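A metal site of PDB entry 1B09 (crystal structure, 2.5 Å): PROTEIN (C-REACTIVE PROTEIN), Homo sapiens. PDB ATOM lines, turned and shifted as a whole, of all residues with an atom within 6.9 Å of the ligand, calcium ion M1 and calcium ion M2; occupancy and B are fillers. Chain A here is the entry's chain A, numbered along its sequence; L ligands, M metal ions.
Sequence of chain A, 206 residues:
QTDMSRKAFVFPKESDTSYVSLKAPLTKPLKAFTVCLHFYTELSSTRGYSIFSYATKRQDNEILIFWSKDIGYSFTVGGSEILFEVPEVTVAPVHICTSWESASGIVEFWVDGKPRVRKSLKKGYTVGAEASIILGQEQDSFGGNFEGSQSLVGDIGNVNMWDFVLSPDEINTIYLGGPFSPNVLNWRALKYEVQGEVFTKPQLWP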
ATOM      1  N   SER A  53       9.841 -15.202  13.276  1.00  0.00           N
ATOM      2  CA  SER A  53      11.087 -14.896  14.001  1.00  0.00           C
ATOM      3  C   SER A  53      12.262 -15.799  13.652  1.00  0.00           C
ATOM      4  O   SER A  53      12.337 -16.983  14.077  1.00  0.00           O
ATOM      5  CB  SER A  53      10.791 -14.984  15.506  1.00  0.00           C
ATOM      6  OG  SER A  53      11.924 -14.496  16.231  1.00  0.00           O
ATOM      7  N   GLN A  59      22.825 -13.274  16.764  1.00  0.00           N
ATOM      8  CA  GLN A  59      21.882 -12.172  16.486  1.00  0.00           C
ATOM      9  C   GLN A  59      20.409 -12.608  16.568  1.00  0.00           C
ATOM     10  O   GLN A  59      19.884 -13.337  15.691  1.00  0.00           O
ATOM     11  CB  GLN A  59      22.217 -11.648  15.086  1.00  0.00           C
ATOM     12  CG  GLN A  59      21.133 -10.766  14.487  1.00  0.00           C
ATOM     13  CD  GLN A  59      21.092  -9.456  15.232  1.00  0.00           C
ATOM     14  OE1 GLN A  59      20.229  -9.190  16.051  1.00  0.00           O
ATOM     15  NE2 GLN A  59      22.095  -8.613  14.921  1.00  0.00           N
ATOM     16  N   ASP A  60      19.733 -12.175  17.667  1.00  0.00           N
ATOM     17  CA  ASP A  60      18.361 -12.680  17.935  1.00  0.00           C
ATOM     18  C   ASP A  60      17.300 -12.127  16.999  1.00  0.00           C
ATOM     19  O   ASP A  60      16.138 -12.584  17.002  1.00  0.00           O
ATOM     20  CB  ASP A  60      17.995 -12.325  19.381  1.00  0.00           C
ATOM     21  CG  ASP A  60      17.963 -10.819  19.545  1.00  0.00           C
ATOM     22  OD1 ASP A  60      18.101 -10.127  18.531  1.00  0.00           O
ATOM     23  OD2 ASP A  60      17.798 -10.354  20.661  1.00  0.00           O
ATOM     24  N   ASN A  61      17.685 -11.104  16.218  1.00  0.00           N
ATOM     25  CA  ASN A  61      16.798 -10.639  15.171  1.00  0.00           C
ATOM     26  C   ASN A  61      17.430 -10.716  13.794  1.00  0.00           C
ATOM     27  O   ASN A  61      17.487  -9.703  13.065  1.00  0.00           O
ATOM     28  CB  ASN A  61      16.457  -9.199  15.479  1.00  0.00           C
ATOM     29  CG  ASN A  61      15.549  -9.138  16.670  1.00  0.00           C
ATOM     30  OD1 ASN A  61      15.039 -10.134  17.152  1.00  0.00           O
ATOM     31  ND2 ASN A  61      15.350  -7.894  17.141  1.00  0.00           N
ATOM     32  N   LEU A  64      13.228 -10.560  11.282  1.00  0.00           N
ATOM     33  CA  LEU A  64      12.006 -10.514  12.060  1.00  0.00           C
ATOM     34  C   LEU A  64      10.923  -9.700  11.351  1.00  0.00           C
ATOM     35  O   LEU A  64      11.192  -8.590  10.810  1.00  0.00           O
ATOM     36  CB  LEU A  64      12.336  -9.848  13.412  1.00  0.00           C
ATOM     37  CG  LEU A  64      11.158  -9.777  14.372  1.00  0.00           C
ATOM     38  CD1 LEU A  64      10.939 -11.091  15.124  1.00  0.00           C
ATOM     39  CD2 LEU A  64      11.374  -8.729  15.463  1.00  0.00           C
ATOM     40  N   PHE A  66       7.262  -7.971  12.294  1.00  0.00           N
ATOM     41  CA  PHE A  66       6.605  -7.616  13.556  1.00  0.00           C
ATOM     42  C   PHE A  66       5.552  -6.551  13.374  1.00  0.00           C
ATOM     43  O   PHE A  66       5.721  -5.588  12.569  1.00  0.00           O
ATOM     44  CB  PHE A  66       7.719  -7.084  14.475  1.00  0.00           C
ATOM     45  CG  PHE A  66       7.288  -7.117  15.934  1.00  0.00           C
ATOM     46  CD1 PHE A  66       7.569  -8.237  16.705  1.00  0.00           C
ATOM     47  CD2 PHE A  66       6.707  -6.000  16.517  1.00  0.00           C
ATOM     48  CE1 PHE A  66       7.270  -8.227  18.067  1.00  0.00           C
ATOM     49  CE2 PHE A  66       6.407  -6.002  17.872  1.00  0.00           C
ATOM     50  CZ  PHE A  66       6.682  -7.116  18.648  1.00  0.00           C
ATOM     51  N   TRP A  67       4.419  -6.712  14.084  1.00  0.00           N
ATOM     52  CA  TRP A  67       3.451  -5.633  14.115  1.00  0.00           C
ATOM     53  C   TRP A  67       3.554  -4.813  15.380  1.00  0.00           C
ATOM     54  O   TRP A  67       3.331  -5.334  16.512  1.00  0.00           O
ATOM     55  CB  TRP A  67       2.054  -6.241  14.023  1.00  0.00           C
ATOM     56  CG  TRP A  67       1.014  -5.147  14.231  1.00  0.00           C
ATOM     57  CD1 TRP A  67       0.395  -4.803  15.454  1.00  0.00           C
ATOM     58  CD2 TRP A  67       0.414  -4.277  13.217  1.00  0.00           C
ATOM     59  NE1 TRP A  67      -0.530  -3.816  15.318  1.00  0.00           N
ATOM     60  CE2 TRP A  67      -0.549  -3.470  13.877  1.00  0.00           C
ATOM     61  CE3 TRP A  67       0.586  -4.130  11.844  1.00  0.00           C
ATOM     62  CZ2 TRP A  67      -1.282  -2.534  13.165  1.00  0.00           C
ATOM     63  CZ3 TRP A  67      -0.155  -3.201  11.129  1.00  0.00           C
ATOM     64  CH2 TRP A  67      -1.102  -2.397  11.796  1.00  0.00           C
ATOM     65  N   SER A  68       3.957  -3.543  15.221  1.00  0.00           N
ATOM     66  CA  SER A  68       3.902  -2.613  16.360  1.00  0.00           C
ATOM     67  C   SER A  68       2.648  -1.771  16.350  1.00  0.00           C
ATOM     68  O   SER A  68       2.344  -1.037  15.371  1.00  0.00           O
ATOM     69  CB  SER A  68       5.136  -1.726  16.285  1.00  0.00           C
ATOM     70  OG  SER A  68       5.412  -1.419  14.913  1.00  0.00           O
ATOM     71  N   SER A  74       6.710  -3.722  11.115  1.00  0.00           N
ATOM     72  CA  SER A  74       8.141  -3.536  11.356  1.00  0.00           C
ATOM     73  C   SER A  74       8.962  -4.687  10.820  1.00  0.00           C
ATOM     74  O   SER A  74       8.681  -5.886  11.089  1.00  0.00           O
ATOM     75  CB  SER A  74       8.327  -3.420  12.865  1.00  0.00           C
ATOM     76  OG  SER A  74       9.623  -3.916  13.220  1.00  0.00           O
ATOM     77  N   PHE A  75      10.008  -4.338  10.014  1.00  0.00           N
ATOM     78  CA  PHE A  75      10.794  -5.366   9.321  1.00  0.00           C
ATOM     79  C   PHE A  75      12.295  -5.217   9.538  1.00  0.00           C
ATOM     80  O   PHE A  75      12.907  -4.184   9.114  1.00  0.00           O
ATOM     81  CB  PHE A  75      10.470  -5.243   7.816  1.00  0.00           C
ATOM     82  CG  PHE A  75      11.265  -6.257   7.013  1.00  0.00           C
ATOM     83  CD1 PHE A  75      11.160  -7.615   7.281  1.00  0.00           C
ATOM     84  CD2 PHE A  75      12.079  -5.805   5.986  1.00  0.00           C
ATOM     85  CE1 PHE A  75      11.881  -8.528   6.505  1.00  0.00           C
ATOM     86  CE2 PHE A  75      12.802  -6.724   5.218  1.00  0.00           C
ATOM     87  CZ  PHE A  75      12.702  -8.082   5.473  1.00  0.00           C
ATOM     88  N   THR A  76      12.891  -6.195  10.231  1.00  0.00           N
ATOM     89  CA  THR A  76      14.326  -6.074  10.515  1.00  0.00           C
ATOM     90  C   THR A  76      15.140  -7.270  10.084  1.00  0.00           C
ATOM     91  O   THR A  76      14.791  -8.451  10.341  1.00  0.00           O
ATOM     92  CB  THR A  76      14.497  -5.862  12.012  1.00  0.00           C
ATOM     93  OG1 THR A  76      15.500  -6.747  12.521  1.00  0.00           O
ATOM     94  CG2 THR A  76      13.180  -6.107  12.748  1.00  0.00           C
ATOM     95  N   GLY A  79      19.407  -7.181  12.736  1.00  0.00           N
ATOM     96  CA  GLY A  79      19.381  -6.254  13.879  1.00  0.00           C
ATOM     97  C   GLY A  79      18.841  -4.874  13.548  1.00  0.00           C
ATOM     98  O   GLY A  79      18.482  -4.082  14.460  1.00  0.00           O
ATOM     99  N   GLU A  81      16.280  -2.022  11.795  1.00  0.00           N
ATOM    100  CA  GLU A  81      14.853  -1.927  11.518  1.00  0.00           C
ATOM    101  C   GLU A  81      14.504  -0.951  10.418  1.00  0.00           C
ATOM    102  O   GLU A  81      15.190   0.114  10.233  1.00  0.00           O
ATOM    103  CB  GLU A  81      14.157  -1.501  12.829  1.00  0.00           C
ATOM    104  CG  GLU A  81      12.650  -1.804  12.853  1.00  0.00           C
ATOM    105  CD  GLU A  81      12.096  -1.470  14.246  1.00  0.00           C
ATOM    106  OE1 GLU A  81      12.843  -1.558  15.212  1.00  0.00           O
ATOM    107  OE2 GLU A  81      10.917  -1.124  14.343  1.00  0.00           O
ATOM    108  N   LEU A  83      10.501   0.640   8.720  1.00  0.00           N
ATOM    109  CA  LEU A  83       9.044   0.582   8.924  1.00  0.00           C
ATOM    110  C   LEU A  83       8.232   0.731   7.642  1.00  0.00           C
ATOM    111  O   LEU A  83       8.575   1.513   6.731  1.00  0.00           O
ATOM    112  CB  LEU A  83       8.642   1.707   9.885  1.00  0.00           C
ATOM    113  CG  LEU A  83       9.222   1.560  11.276  1.00  0.00           C
ATOM    114  CD1 LEU A  83       9.005   2.802  12.148  1.00  0.00           C
ATOM    115  CD2 LEU A  83       8.606   0.382  12.038  1.00  0.00           C
ATOM    116  N   GLU A 138       8.371 -14.632  20.159  1.00  0.00           N
ATOM    117  CA  GLU A 138       9.542 -13.872  19.741  1.00  0.00           C
ATOM    118  C   GLU A 138      10.803 -14.308  20.421  1.00  0.00           C
ATOM    119  O   GLU A 138      10.852 -14.474  21.689  1.00  0.00           O
ATOM    120  CB  GLU A 138       9.287 -12.381  20.026  1.00  0.00           C
ATOM    121  CG  GLU A 138      10.021 -11.470  19.013  1.00  0.00           C
ATOM    122  CD  GLU A 138      11.495 -11.337  19.401  1.00  0.00           C
ATOM    123  OE1 GLU A 138      11.788 -11.218  20.572  1.00  0.00           O
ATOM    124  OE2 GLU A 138      12.340 -11.355  18.495  1.00  0.00           O
ATOM    125  N   GLN A 139      11.837 -14.559  19.598  1.00  0.00           N
ATOM    126  CA  GLN A 139      13.086 -15.042  20.147  1.00  0.00           C
ATOM    127  C   GLN A 139      13.971 -13.932  20.640  1.00  0.00           C
ATOM    128  O   GLN A 139      14.204 -12.932  19.924  1.00  0.00           O
ATOM    129  CB  GLN A 139      13.800 -15.820  19.051  1.00  0.00           C
ATOM    130  CG  GLN A 139      13.251 -17.241  18.883  1.00  0.00           C
ATOM    131  CD  GLN A 139      13.803 -17.861  17.619  1.00  0.00           C
ATOM    132  OE1 GLN A 139      13.673 -17.349  16.521  1.00  0.00           O
ATOM    133  NE2 GLN A 139      14.442 -19.029  17.817  1.00  0.00           N
ATOM    134  N   ASP A 140      14.488 -14.079  21.879  1.00  0.00           N
ATOM    135  CA  ASP A 140      15.591 -13.229  22.315  1.00  0.00           C
ATOM    136  C   ASP A 140      16.881 -14.014  22.480  1.00  0.00           C
ATOM    137  O   ASP A 140      17.962 -13.448  22.803  1.00  0.00           O
ATOM    138  CB  ASP A 140      15.191 -12.585  23.643  1.00  0.00           C
ATOM    139  CG  ASP A 140      14.118 -11.558  23.373  1.00  0.00           C
ATOM    140  OD1 ASP A 140      14.183 -10.926  22.327  1.00  0.00           O
ATOM    141  OD2 ASP A 140      13.221 -11.411  24.200  1.00  0.00           O
ATOM    142  N   SER A 141      16.758 -15.352  22.317  1.00  0.00           N
ATOM    143  CA  SER A 141      17.942 -16.214  22.166  1.00  0.00           C
ATOM    144  C   SER A 141      17.633 -17.424  21.306  1.00  0.00           C
ATOM    145  O   SER A 141      16.458 -17.740  20.995  1.00  0.00           O
ATOM    146  CB  SER A 141      18.392 -16.662  23.563  1.00  0.00           C
ATOM    147  OG  SER A 141      17.551 -17.729  24.015  1.00  0.00           O
ATOM    148  N   ASN A 145      13.875 -17.755  25.258  1.00  0.00           N
ATOM    149  CA  ASN A 145      13.633 -16.428  25.844  1.00  0.00           C
ATOM    150  C   ASN A 145      12.477 -15.730  25.213  1.00  0.00           C
ATOM    151  O   ASN A 145      12.621 -14.709  24.493  1.00  0.00           O
ATOM    152  CB  ASN A 145      14.919 -15.618  25.702  1.00  0.00           C
ATOM    153  CG  ASN A 145      15.921 -16.097  26.740  1.00  0.00           C
ATOM    154  OD1 ASN A 145      16.818 -16.877  26.462  1.00  0.00           O
ATOM    155  ND2 ASN A 145      15.724 -15.607  27.971  1.00  0.00           N
ATOM    156  N   PHE A 146      11.278 -16.292  25.457  1.00  0.00           N
ATOM    157  CA  PHE A 146      10.061 -15.700  24.930  1.00  0.00           C
ATOM    158  C   PHE A 146       9.432 -14.684  25.864  1.00  0.00           C
ATOM    159  O   PHE A 146       9.403 -14.887  27.127  1.00  0.00           O
ATOM    160  CB  PHE A 146       9.056 -16.833  24.696  1.00  0.00           C
ATOM    161  CG  PHE A 146       9.655 -17.898  23.822  1.00  0.00           C
ATOM    162  CD1 PHE A 146      10.513 -17.554  22.794  1.00  0.00           C
ATOM    163  CD2 PHE A 146       9.308 -19.230  24.028  1.00  0.00           C
ATOM    164  CE1 PHE A 146      11.020 -18.536  21.964  1.00  0.00           C
ATOM    165  CE2 PHE A 146       9.823 -20.205  23.200  1.00  0.00           C
ATOM    166  CZ  PHE A 146      10.687 -19.866  22.168  1.00  0.00           C
ATOM    167  N   GLU A 147       8.993 -13.668  25.182  1.00  0.00           N
ATOM    168  CA  GLU A 147       8.116 -12.757  25.885  1.00  0.00           C
ATOM    169  C   GLU A 147       6.643 -13.062  25.597  1.00  0.00           C
ATOM    170  O   GLU A 147       6.155 -12.823  24.439  1.00  0.00           O
ATOM    171  CB  GLU A 147       8.517 -11.271  25.464  1.00  0.00           C
ATOM    172  CG  GLU A 147       9.979 -10.852  25.938  1.00  0.00           C
ATOM    173  CD  GLU A 147      10.187  -9.289  25.932  1.00  0.00           C
ATOM    174  OE1 GLU A 147       9.418  -8.599  26.589  1.00  0.00           O
ATOM    175  OE2 GLU A 147      11.123  -8.830  25.283  1.00  0.00           O
ATOM    176  N   GLN A 150       4.666 -10.423  23.432  1.00  0.00           N
ATOM    177  CA  GLN A 150       4.956 -10.382  21.996  1.00  0.00           C
ATOM    178  C   GLN A 150       4.296 -11.538  21.288  1.00  0.00           C
ATOM    179  O   GLN A 150       4.402 -11.724  20.029  1.00  0.00           O
ATOM    180  CB  GLN A 150       6.488 -10.414  21.817  1.00  0.00           C
ATOM    181  CG  GLN A 150       7.119  -8.996  21.872  1.00  0.00           C
ATOM    182  CD  GLN A 150       8.613  -9.077  22.121  1.00  0.00           C
ATOM    183  OE1 GLN A 150       9.116  -9.795  22.962  1.00  0.00           O
ATOM    184  NE2 GLN A 150       9.339  -8.260  21.314  1.00  0.00           N
HETATM  185  P1  LIG L   1      12.991  -7.926  20.771  1.00  0.00           P
HETATM  186  O1  LIG L   1      13.316  -9.036  19.705  1.00  0.00           O
HETATM  187  O2  LIG L   1      12.255  -8.860  21.724  1.00  0.00           O
HETATM  188  O3  LIG L   1      14.348  -7.665  21.411  1.00  0.00           O
HETATM  189  O4  LIG L   1      12.068  -6.657  20.468  1.00  0.00           O
HETATM  190  C1  LIG L   1      12.051  -5.959  19.184  1.00  0.00           C
HETATM  191  C2  LIG L   1      10.936  -4.883  18.857  1.00  0.00           C
HETATM  192  N1  LIG L   1      10.925  -4.057  17.576  1.00  0.00           N
HETATM  193  C3  LIG L   1      12.242  -4.194  16.936  1.00  0.00           C
HETATM  194  C4  LIG L   1      10.417  -2.630  17.489  1.00  0.00           C
HETATM  195  C5  LIG L   1       9.955  -4.670  16.661  1.00  0.00           C
HETATM  196 CA    CA M   1      14.617 -10.276  19.709  1.00  0.00          CA
HETATM  197 CA    CA M   2      11.581 -10.044  22.813  1.00  0.00          CA
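Calcium ion M2 is bound by an oxygen (O2) of the ligand (1.7 Å), the side-chain amide oxygen (OE1) of Gln 150 (2.5 Å), the side-chain carboxylate (OE1) of Glu 138 (2.5 Å), the side-chain carboxylate (OD2) of Asp 140 (2.5 Å), the side-chain carboxylate (OE2) of Glu 147 (2.8 Å) and the side-chain carboxylate (OD1) of Asp 140 (2.8 Å).
OE1 of Glu 81 lies within salt-bridge range of N1 of the ligand, at 3.9 Å.
The backbone NH (N) of Asn 61 sits close to the side-chain amide oxygen (OE1) of Gln 59. O of Asn 145 lies within hydrogen-bond range of N of Asp 140 (3.3 Å). O of Phe 66 lies within hydrogen-bond range of N of Ser 74. The side-chain amide oxygen (OE1) of Gln 139 lies close to the backbone carbonyl oxygen (O) of Ser 53. The backbone carbonyl oxygen of Asn 61 lies within hydrogen-bond range of the backbone NH of Gly 79 (3.2 Å). OD1 of Asn 61 lies close to OD1 of Asp 60, at 3.4 Å. The side-chain amide oxygen (OE1) of Gln 59 sits close to the side-chain carboxylate (OD1) of Asp 60 (3.4 Å). The side-chain hydroxyl of Ser 74 is in hydrogen-bond range of the side-chain carboxylate of Glu 81 (3.3 Å).
Calcium ion M1 is bound by O1 of the ligand (1.8 Å), OD1 of Asn 61 (2.6 Å), O of Gln 139 (2.7 Å), OD1 of Asp 140 (2.7 Å) and OE2 of Glu 138 (2.8 Å). Calcium ion M1 has five donor atoms within binding distance. Slightly farther from calcium ion M1 lies the side-chain carboxylate (OE1) of Glu 138 (3.1 Å). Slightly farther from calcium ion M1 lies O3 of the ligand (3.1 Å).
Within 4 Å of calcium ion M2: Glu 138, Asp 140, Glu 147 and Gln 150. The nearest printed residue that does not touch calcium ion M2 is Gln 139 (4.9 Å).
Residues that only touch the ligand: Phe 66 (3.5 Å) and Ser 74 (3.5 Å). Hydrophobic or aromatic side chains that line the ligand: Phe 66. Eight residues have an atom within 4 Å of the ligand: Asn 61, Phe 66, Ser 74, Glu 81, Glu 138, Asp 140, Glu 147 and Gln 150. The nearest printed residue that does not touch the ligand is Gln 139 (4.002 Å).
OD2 of Asp 60 touches calcium ion M1, at 3.3 Å. Of the 22 residues printed, 5 come within 4 Å of calcium ion M1. The nearest printed residue that does not touch calcium ion M1 is Leu 64 (5.6 Å).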
